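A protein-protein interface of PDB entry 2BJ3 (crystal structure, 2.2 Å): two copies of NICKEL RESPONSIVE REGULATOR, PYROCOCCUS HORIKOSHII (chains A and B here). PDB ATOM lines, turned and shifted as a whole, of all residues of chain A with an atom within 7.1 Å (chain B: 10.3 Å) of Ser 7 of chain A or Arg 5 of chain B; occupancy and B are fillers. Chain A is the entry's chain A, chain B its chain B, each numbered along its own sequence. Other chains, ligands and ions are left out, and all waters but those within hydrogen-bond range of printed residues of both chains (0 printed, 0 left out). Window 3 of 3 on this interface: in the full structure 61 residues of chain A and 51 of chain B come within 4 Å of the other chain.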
ATOM      1  N   ARG A   5       4.747 -17.332 -16.141  1.00  0.00           N
ATOM      2  CA  ARG A   5       3.889 -18.377 -15.587  1.00  0.00           C
ATOM      3  C   ARG A   5       4.640 -19.684 -15.416  1.00  0.00           C
ATOM      4  O   ARG A   5       5.310 -20.144 -16.341  1.00  0.00           O
ATOM      5  CB  ARG A   5       2.682 -18.632 -16.489  1.00  0.00           C
ATOM      6  CG  ARG A   5       1.363 -18.579 -15.751  1.00  0.00           C
ATOM      7  CD  ARG A   5       0.226 -19.213 -16.535  1.00  0.00           C
ATOM      8  NE  ARG A   5      -1.080 -18.856 -15.976  1.00  0.00           N
ATOM      9  CZ  ARG A   5      -1.418 -18.994 -14.695  1.00  0.00           C
ATOM     10  NH1 ARG A   5      -0.552 -19.483 -13.821  1.00  0.00           N
ATOM     11  NH2 ARG A   5      -2.628 -18.641 -14.281  1.00  0.00           N
ATOM     12  N   PHE A   6       4.546 -20.262 -14.222  1.00  0.00           N
ATOM     13  CA  PHE A   6       5.176 -21.546 -13.926  1.00  0.00           C
ATOM     14  C   PHE A   6       4.354 -22.294 -12.868  1.00  0.00           C
ATOM     15  O   PHE A   6       3.449 -21.724 -12.252  1.00  0.00           O
ATOM     16  CB  PHE A   6       6.646 -21.364 -13.493  1.00  0.00           C
ATOM     17  CG  PHE A   6       6.836 -20.671 -12.164  1.00  0.00           C
ATOM     18  CD1 PHE A   6       7.070 -21.413 -11.001  1.00  0.00           C
ATOM     19  CD2 PHE A   6       6.811 -19.278 -12.075  1.00  0.00           C
ATOM     20  CE1 PHE A   6       7.276 -20.777  -9.773  1.00  0.00           C
ATOM     21  CE2 PHE A   6       7.013 -18.634 -10.855  1.00  0.00           C
ATOM     22  CZ  PHE A   6       7.248 -19.384  -9.699  1.00  0.00           C
ATOM     23  N   SER A   7       4.642 -23.577 -12.679  1.00  0.00           N
ATOM     24  CA  SER A   7       3.894 -24.364 -11.714  1.00  0.00           C
ATOM     25  C   SER A   7       4.782 -24.894 -10.611  1.00  0.00           C
ATOM     26  O   SER A   7       5.983 -25.080 -10.800  1.00  0.00           O
ATOM     27  CB  SER A   7       3.175 -25.523 -12.412  1.00  0.00           C
ATOM     28  OG  SER A   7       4.085 -26.376 -13.072  1.00  0.00           O
ATOM     29  N   ILE A   8       4.175 -25.139  -9.456  1.00  0.00           N
ATOM     30  CA  ILE A   8       4.901 -25.639  -8.299  1.00  0.00           C
ATOM     31  C   ILE A   8       4.075 -26.725  -7.583  1.00  0.00           C
ATOM     32  O   ILE A   8       2.848 -26.765  -7.715  1.00  0.00           O
ATOM     33  CB  ILE A   8       5.173 -24.487  -7.319  1.00  0.00           C
ATOM     34  CG1 ILE A   8       3.843 -23.821  -6.941  1.00  0.00           C
ATOM     35  CG2 ILE A   8       6.100 -23.460  -7.961  1.00  0.00           C
ATOM     36  CD1 ILE A   8       3.946 -22.824  -5.805  1.00  0.00           C
ATOM     37  N   SER A   9       4.742 -27.600  -6.836  1.00  0.00           N
ATOM     38  CA  SER A   9       4.046 -28.656  -6.101  1.00  0.00           C
ATOM     39  C   SER A   9       4.132 -28.408  -4.601  1.00  0.00           C
ATOM     40  O   SER A   9       5.220 -28.377  -4.030  1.00  0.00           O
ATOM     41  CB  SER A   9       4.639 -30.024  -6.428  1.00  0.00           C
ATOM     42  OG  SER A   9       4.249 -30.449  -7.726  1.00  0.00           O
ATOM     43  N   ILE A  10       2.975 -28.228  -3.973  1.00  0.00           N
ATOM     44  CA  ILE A  10       2.893 -27.965  -2.538  1.00  0.00           C
ATOM     45  C   ILE A  10       1.919 -28.932  -1.878  1.00  0.00           C
ATOM     46  O   ILE A  10       0.811 -29.128  -2.363  1.00  0.00           O
ATOM     47  CB  ILE A  10       2.392 -26.520  -2.268  1.00  0.00           C
ATOM     48  CG1 ILE A  10       3.338 -25.506  -2.924  1.00  0.00           C
ATOM     49  CG2 ILE A  10       2.273 -26.268  -0.761  1.00  0.00           C
ATOM     50  CD1 ILE A  10       4.752 -25.555  -2.412  1.00  0.00           C
ATOM     51  N   LEU A  15      -1.354 -26.185   1.585  1.00  0.00           N
ATOM     52  CA  LEU A  15      -2.061 -25.379   0.601  1.00  0.00           C
ATOM     53  C   LEU A  15      -3.491 -25.088   1.012  1.00  0.00           C
ATOM     54  O   LEU A  15      -4.011 -24.008   0.746  1.00  0.00           O
ATOM     55  CB  LEU A  15      -2.043 -26.072  -0.766  1.00  0.00           C
ATOM     56  CG  LEU A  15      -2.537 -25.246  -1.964  1.00  0.00           C
ATOM     57  CD1 LEU A  15      -1.591 -24.061  -2.195  1.00  0.00           C
ATOM     58  CD2 LEU A  15      -2.605 -26.125  -3.214  1.00  0.00           C
ATOM     59  N   ARG A  30      -3.630 -16.842  -5.177  1.00  0.00           N
ATOM     60  CA  ARG A  30      -2.360 -17.359  -4.675  1.00  0.00           C
ATOM     61  C   ARG A  30      -1.148 -16.621  -5.230  1.00  0.00           C
ATOM     62  O   ARG A  30      -0.175 -16.392  -4.514  1.00  0.00           O
ATOM     63  CB  ARG A  30      -2.214 -18.827  -5.033  1.00  0.00           C
ATOM     64  CG  ARG A  30      -3.152 -19.751  -4.331  1.00  0.00           C
ATOM     65  CD  ARG A  30      -3.156 -21.066  -5.062  1.00  0.00           C
ATOM     66  NE  ARG A  30      -4.002 -22.050  -4.413  1.00  0.00           N
ATOM     67  CZ  ARG A  30      -4.486 -23.128  -5.024  1.00  0.00           C
ATOM     68  NH1 ARG A  30      -4.204 -23.350  -6.304  1.00  0.00           N
ATOM     69  NH2 ARG A  30      -5.244 -23.986  -4.351  1.00  0.00           N
ATOM     70  N   GLU B   2       0.668 -36.517  -1.605  1.00  0.00           N
ATOM     71  CA  GLU B   2      -0.195 -35.481  -0.970  1.00  0.00           C
ATOM     72  C   GLU B   2       0.057 -34.122  -1.624  1.00  0.00           C
ATOM     73  O   GLU B   2      -0.531 -33.114  -1.240  1.00  0.00           O
ATOM     74  CB  GLU B   2       0.120 -35.387   0.522  1.00  0.00           C
ATOM     75  CG  GLU B   2      -0.791 -34.440   1.268  1.00  0.00           C
ATOM     76  CD  GLU B   2      -0.047 -33.579   2.263  1.00  0.00           C
ATOM     77  OE1 GLU B   2      -0.709 -32.778   2.960  1.00  0.00           O
ATOM     78  OE2 GLU B   2       1.197 -33.702   2.339  1.00  0.00           O
ATOM     79  N   LEU B   3       0.932 -34.110  -2.622  1.00  0.00           N
ATOM     80  CA  LEU B   3       1.294 -32.884  -3.319  1.00  0.00           C
ATOM     81  C   LEU B   3       0.278 -32.382  -4.342  1.00  0.00           C
ATOM     82  O   LEU B   3      -0.230 -33.148  -5.162  1.00  0.00           O
ATOM     83  CB  LEU B   3       2.642 -33.067  -4.019  1.00  0.00           C
ATOM     84  CG  LEU B   3       3.861 -33.380  -3.152  1.00  0.00           C
ATOM     85  CD1 LEU B   3       5.089 -33.508  -4.042  1.00  0.00           C
ATOM     86  CD2 LEU B   3       4.067 -32.284  -2.123  1.00  0.00           C
ATOM     87  N   ILE B   4      -0.020 -31.088  -4.285  1.00  0.00           N
ATOM     88  CA  ILE B   4      -0.931 -30.471  -5.243  1.00  0.00           C
ATOM     89  C   ILE B   4      -0.059 -29.607  -6.164  1.00  0.00           C
ATOM     90  O   ILE B   4       0.808 -28.859  -5.700  1.00  0.00           O
ATOM     91  CB  ILE B   4      -1.955 -29.543  -4.564  1.00  0.00           C
ATOM     92  CG1 ILE B   4      -2.833 -30.332  -3.575  1.00  0.00           C
ATOM     93  CG2 ILE B   4      -2.794 -28.842  -5.638  1.00  0.00           C
ATOM     94  CD1 ILE B   4      -3.822 -31.311  -4.202  1.00  0.00           C
ATOM     95  N   ARG B   5      -0.259 -29.719  -7.467  1.00  0.00           N
ATOM     96  CA  ARG B   5       0.521 -28.903  -8.381  1.00  0.00           C
ATOM     97  C   ARG B   5      -0.339 -27.810  -8.954  1.00  0.00           C
ATOM     98  O   ARG B   5      -1.443 -28.069  -9.425  1.00  0.00           O
ATOM     99  CB  ARG B   5       1.094 -29.726  -9.525  1.00  0.00           C
ATOM    100  CG  ARG B   5       1.562 -28.855 -10.673  1.00  0.00           C
ATOM    101  CD  ARG B   5       2.565 -29.567 -11.544  1.00  0.00           C
ATOM    102  NE  ARG B   5       3.704 -29.976 -10.741  1.00  0.00           N
ATOM    103  CZ  ARG B   5       4.856 -30.390 -11.241  1.00  0.00           C
ATOM    104  NH1 ARG B   5       5.027 -30.449 -12.555  1.00  0.00           N
ATOM    105  NH2 ARG B   5       5.835 -30.745 -10.424  1.00  0.00           N
ATOM    106  N   PHE B   6       0.164 -26.583  -8.909  1.00  0.00           N
ATOM    107  CA  PHE B   6      -0.582 -25.465  -9.451  1.00  0.00           C
ATOM    108  C   PHE B   6       0.322 -24.445 -10.138  1.00  0.00           C
ATOM    109  O   PHE B   6       1.535 -24.410  -9.925  1.00  0.00           O
ATOM    110  CB  PHE B   6      -1.438 -24.797  -8.361  1.00  0.00           C
ATOM    111  CG  PHE B   6      -0.650 -24.272  -7.188  1.00  0.00           C
ATOM    112  CD1 PHE B   6      -0.014 -25.141  -6.311  1.00  0.00           C
ATOM    113  CD2 PHE B   6      -0.573 -22.902  -6.944  1.00  0.00           C
ATOM    114  CE1 PHE B   6       0.684 -24.658  -5.206  1.00  0.00           C
ATOM    115  CE2 PHE B   6       0.121 -22.412  -5.844  1.00  0.00           C
ATOM    116  CZ  PHE B   6       0.750 -23.290  -4.974  1.00  0.00           C
ATOM    117  N   SER B   7      -0.298 -23.623 -10.973  1.00  0.00           N
ATOM    118  CA  SER B   7       0.392 -22.611 -11.759  1.00  0.00           C
ATOM    119  C   SER B   7       0.256 -21.234 -11.107  1.00  0.00           C
ATOM    120  O   SER B   7      -0.824 -20.866 -10.630  1.00  0.00           O
ATOM    121  CB  SER B   7      -0.224 -22.596 -13.170  1.00  0.00           C
ATOM    122  OG  SER B   7       0.560 -21.866 -14.091  1.00  0.00           O
ATOM    123  N   ILE B   8       1.353 -20.484 -11.074  1.00  0.00           N
ATOM    124  CA  ILE B   8       1.335 -19.142 -10.500  1.00  0.00           C
ATOM    125  C   ILE B   8       1.967 -18.125 -11.456  1.00  0.00           C
ATOM    126  O   ILE B   8       2.848 -18.461 -12.256  1.00  0.00           O
ATOM    127  CB  ILE B   8       2.095 -19.072  -9.152  1.00  0.00           C
ATOM    128  CG1 ILE B   8       3.585 -19.304  -9.389  1.00  0.00           C
ATOM    129  CG2 ILE B   8       1.522 -20.103  -8.169  1.00  0.00           C
ATOM    130  CD1 ILE B   8       4.411 -19.228  -8.132  1.00  0.00           C
ATOM    131  N   SER B   9       1.507 -16.882 -11.357  1.00  0.00           N
ATOM    132  CA  SER B   9       2.005 -15.780 -12.179  1.00  0.00           C
ATOM    133  C   SER B   9       2.841 -14.819 -11.330  1.00  0.00           C
ATOM    134  O   SER B   9       2.314 -14.205 -10.409  1.00  0.00           O
ATOM    135  CB  SER B   9       0.823 -15.029 -12.785  1.00  0.00           C
ATOM    136  OG  SER B   9       1.262 -13.852 -13.437  1.00  0.00           O
ATOM    137  N   ILE B  10       4.136 -14.703 -11.633  1.00  0.00           N
ATOM    138  CA  ILE B  10       5.060 -13.816 -10.907  1.00  0.00           C
ATOM    139  C   ILE B  10       5.788 -12.856 -11.876  1.00  0.00           C
ATOM    140  O   ILE B  10       6.196 -13.264 -12.962  1.00  0.00           O
ATOM    141  CB  ILE B  10       6.148 -14.633 -10.174  1.00  0.00           C
ATOM    142  CG1 ILE B  10       5.505 -15.631  -9.204  1.00  0.00           C
ATOM    143  CG2 ILE B  10       7.100 -13.710  -9.447  1.00  0.00           C
ATOM    144  CD1 ILE B  10       4.641 -15.015  -8.107  1.00  0.00           C
ATOM    145  N   LEU B  15      11.114 -12.837 -10.129  1.00  0.00           N
ATOM    146  CA  LEU B  15      11.485 -14.226 -10.336  1.00  0.00           C
ATOM    147  C   LEU B  15      12.995 -14.372 -10.495  1.00  0.00           C
ATOM    148  O   LEU B  15      13.580 -15.328  -9.998  1.00  0.00           O
ATOM    149  CB  LEU B  15      10.752 -14.772 -11.567  1.00  0.00           C
ATOM    150  CG  LEU B  15      10.730 -16.286 -11.814  1.00  0.00           C
ATOM    151  CD1 LEU B  15      10.402 -17.048 -10.524  1.00  0.00           C
ATOM    152  CD2 LEU B  15       9.683 -16.573 -12.859  1.00  0.00           C
ATOM    153  N   PHE B  18      14.501 -13.841  -7.244  1.00  0.00           N
ATOM    154  CA  PHE B  18      14.124 -14.997  -6.430  1.00  0.00           C
ATOM    155  C   PHE B  18      15.027 -16.177  -6.776  1.00  0.00           C
ATOM    156  O   PHE B  18      15.649 -16.764  -5.892  1.00  0.00           O
ATOM    157  CB  PHE B  18      12.654 -15.370  -6.652  1.00  0.00           C
ATOM    158  CG  PHE B  18      12.176 -16.505  -5.774  1.00  0.00           C
ATOM    159  CD1 PHE B  18      12.280 -16.425  -4.392  1.00  0.00           C
ATOM    160  CD2 PHE B  18      11.639 -17.657  -6.332  1.00  0.00           C
ATOM    161  CE1 PHE B  18      11.860 -17.473  -3.575  1.00  0.00           C
ATOM    162  CE2 PHE B  18      11.215 -18.713  -5.523  1.00  0.00           C
ATOM    163  CZ  PHE B  18      11.329 -18.618  -4.143  1.00  0.00           C
ATOM    164  N   ASP B  19      15.116 -16.524  -8.059  1.00  0.00           N
ATOM    165  CA  ASP B  19      15.984 -17.635  -8.471  1.00  0.00           C
ATOM    166  C   ASP B  19      17.417 -17.349  -8.039  1.00  0.00           C
ATOM    167  O   ASP B  19      18.141 -18.245  -7.604  1.00  0.00           O
ATOM    168  CB  ASP B  19      15.944 -17.838  -9.990  1.00  0.00           C
ATOM    169  CG  ASP B  19      14.596 -18.324 -10.481  1.00  0.00           C
ATOM    170  OD1 ASP B  19      13.956 -19.118  -9.756  1.00  0.00           O
ATOM    171  OD2 ASP B  19      14.181 -17.925 -11.595  1.00  0.00           O
ATOM    172  N   ASN B  29      14.920 -26.236  -5.710  1.00  0.00           N
ATOM    173  CA  ASN B  29      13.955 -25.704  -6.656  1.00  0.00           C
ATOM    174  C   ASN B  29      13.021 -24.682  -6.023  1.00  0.00           C
ATOM    175  O   ASN B  29      13.028 -24.477  -4.809  1.00  0.00           O
ATOM    176  CB  ASN B  29      13.134 -26.853  -7.220  1.00  0.00           C
ATOM    177  CG  ASN B  29      12.507 -27.690  -6.130  1.00  0.00           C
ATOM    178  OD1 ASN B  29      11.563 -27.262  -5.465  1.00  0.00           O
ATOM    179  ND2 ASN B  29      13.045 -28.883  -5.920  1.00  0.00           N
ATOM    180  N   ARG B  30      12.210 -24.053  -6.863  1.00  0.00           N
ATOM    181  CA  ARG B  30      11.260 -23.049  -6.415  1.00  0.00           C
ATOM    182  C   ARG B  30      10.238 -23.626  -5.441  1.00  0.00           C
ATOM    183  O   ARG B  30       9.984 -23.039  -4.390  1.00  0.00           O
ATOM    184  CB  ARG B  30      10.542 -22.463  -7.617  1.00  0.00           C
ATOM    185  CG  ARG B  30      11.439 -21.663  -8.518  1.00  0.00           C
ATOM    186  CD  ARG B  30      10.711 -21.338  -9.793  1.00  0.00           C
ATOM    187  NE  ARG B  30      11.530 -20.542 -10.688  1.00  0.00           N
ATOM    188  CZ  ARG B  30      11.371 -20.515 -12.005  1.00  0.00           C
ATOM    189  NH1 ARG B  30      10.422 -21.249 -12.578  1.00  0.00           N
ATOM    190  NH2 ARG B  30      12.155 -19.747 -12.748  1.00  0.00           N
ATOM    191  N   SER B  31       9.657 -24.769  -5.799  1.00  0.00           N
ATOM    192  CA  SER B  31       8.659 -25.439  -4.965  1.00  0.00           C
ATOM    193  C   SER B  31       9.111 -25.580  -3.521  1.00  0.00           C
ATOM    194  O   SER B  31       8.414 -25.162  -2.601  1.00  0.00           O
ATOM    195  CB  SER B  31       8.349 -26.817  -5.540  1.00  0.00           C
ATOM    196  OG  SER B  31       7.492 -26.709  -6.659  1.00  0.00           O
ATOM    197  N   GLU B  32      10.285 -26.175  -3.341  1.00  0.00           N
ATOM    198  CA  GLU B  32      10.883 -26.386  -2.030  1.00  0.00           C
ATOM    199  C   GLU B  32      11.080 -25.085  -1.241  1.00  0.00           C
ATOM    200  O   GLU B  32      11.004 -25.077  -0.011  1.00  0.00           O
ATOM    201  CB  GLU B  32      12.221 -27.107  -2.210  1.00  0.00           C
ATOM    202  CG  GLU B  32      13.120 -27.142  -0.985  1.00  0.00           C
ATOM    203  CD  GLU B  32      14.390 -27.963  -1.211  1.00  0.00           C
ATOM    204  OE1 GLU B  32      15.091 -27.730  -2.222  1.00  0.00           O
ATOM    205  OE2 GLU B  32      14.690 -28.840  -0.372  1.00  0.00           O
ATOM    206  N   ILE B  34       9.279 -22.027  -1.861  1.00  0.00           N
ATOM    207  CA  ILE B  34       7.969 -21.450  -1.625  1.00  0.00           C
ATOM    208  C   ILE B  34       7.217 -22.227  -0.538  1.00  0.00           C
ATOM    209  O   ILE B  34       6.462 -21.641   0.233  1.00  0.00           O
ATOM    210  CB  ILE B  34       7.182 -21.423  -2.930  1.00  0.00           C
ATOM    211  CG1 ILE B  34       7.852 -20.428  -3.883  1.00  0.00           C
ATOM    212  CG2 ILE B  34       5.728 -21.077  -2.677  1.00  0.00           C
ATOM    213  CD1 ILE B  34       7.216 -20.349  -5.260  1.00  0.00           C
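NH1 of Arg 5 of chain A sits at hydrogen-bond distance from OG of Ser 7 of chain B (2.6 Å).
The backbone carbonyl oxygen (O) of Phe 6 of chain A lies close to the side-chain hydroxyl (OG) of Ser 7 of chain B, 3.4 Å away.
The backbone carbonyl oxygen (O) of Phe 6 of chain A sits at hydrogen-bond distance from the backbone NH (N) of Ile 8 of chain B, 2.7 Å away.
The backbone NH (N) of Ile 8 of chain A sits at hydrogen-bond distance from the backbone carbonyl oxygen (O) of Phe 6 of chain B, at 2.8 Å.
OG of Ser 9 of chain A is in hydrogen-bond range of NE of Arg 5 of chain B, 3.1 Å away.
The backbone NH (N) of Ser 9 of chain A sits at hydrogen-bond distance from the side-chain hydroxyl (OG) of Ser 31 of chain B, 2.9 Å away.
The backbone carbonyl oxygen (O) of Ile 4 of chain B is in hydrogen-bond range of the backbone NH (N) of Ile 10 of chain A (2.8 Å).
The guanidinium group (NH1) of Arg 5 of chain A lies close to the backbone NH (N) of Ile 8 of chain B (3.5 Å).
The side-chain carboxylate of Asp 19 of chain B lies within salt-bridge range of the guanidinium group of Arg 30 of chain B (3.0 Å).
N of Ser 31 of chain B is in hydrogen-bond range of OD1 of Asn 29 of chain B (3.2 Å).
Leu 15 of chain B touches Phe 6 of chain A.
Phe 6 of chain A touches Arg 30 of chain B (CE1 to CD, 3.5 Å).
OG of Ser 7 of chain A touches CD of Arg 5 of chain B (3.9 Å).
CA of Ser 7 of chain A touches CA of Ser 7 of chain B (3.9 Å).
Ile 8 of chain A touches Ile 4 of chain B (O to O, 3.6 Å).
Ile 8 of chain A touches Ser 31 of chain B.
Phe 6 of chain B touches Ile 10 of chain A.
O of Ser 31 of chain B touches CD1 of Ile 10 of chain A, at 3.7 Å.
Ile 4 of chain B touches Leu 15 of chain A (CG2 to CD2, 3.6 Å).
Leu 15 of chain A touches Phe 6 of chain B.
Ser 7 of chain A touches just these residues of chain B: Arg 5, Phe 6 and Ser 7.
Printed residues of chain A within 4 Å of Arg 30 of chain B: Phe 6.
Of the printed residues of chain B, Ile 10 of chain A touches Leu 3, Ile 4, Phe 6 and Ser 31.
Of the printed residues of chain A, Ser 7 of chain B touches Arg 5, Phe 6 and Ser 7.
Of the printed residues of chain B, Leu 15 of chain A touches Ile 4 and Phe 6.
Asn 29 of chain B touches none of the printed residues of chain A.
Ile 34 of chain B touches none of the printed residues of chain A.
The nearest printed residue of chain B that does not touch Ser 7 of chain A is Ile 8 of chain B (4.7 Å).
The nearest printed residue of chain A that does not touch Phe 6 of chain B is Phe 6 of chain A (4.04 Å).
Printed residues of chain B that touch a printed residue of chain A: Leu 3, Ile 4, Arg 5, Phe 6, Ser 7, Ile 8, Ile 10, Leu 15, Arg 30 and Ser 31.
Printed residues of chain A that touch a printed residue of chain B: Arg 5, Phe 6, Ser 7, Ile 8, Ser 9, Ile 10, Leu 15 and Arg 30.
Among the printed residues, 24 pairs touch across the chains.
Among the printed residues, no Asp or Glu carboxylate lies within 4 Å of a Lys or Arg side-chain nitrogen of the other chain.
Arg 5 of chain A touches Ser 7 of chain B, and with the chains exchanged Ser 7 of chain A touches Arg 5 of chain B.
Arg 5 of chain A touches Ile 8 of chain B, and with the chains exchanged Ile 8 of chain A touches Arg 5 of chain B.
Phe 6 of chain A touches Ser 7 of chain B, and with the chains exchanged Ser 7 of chain A touches Phe 6 of chain B.
Phe 6 of chain A touches Leu 15 of chain B, and with the chains exchanged Leu 15 of chain A touches Phe 6 of chain B.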
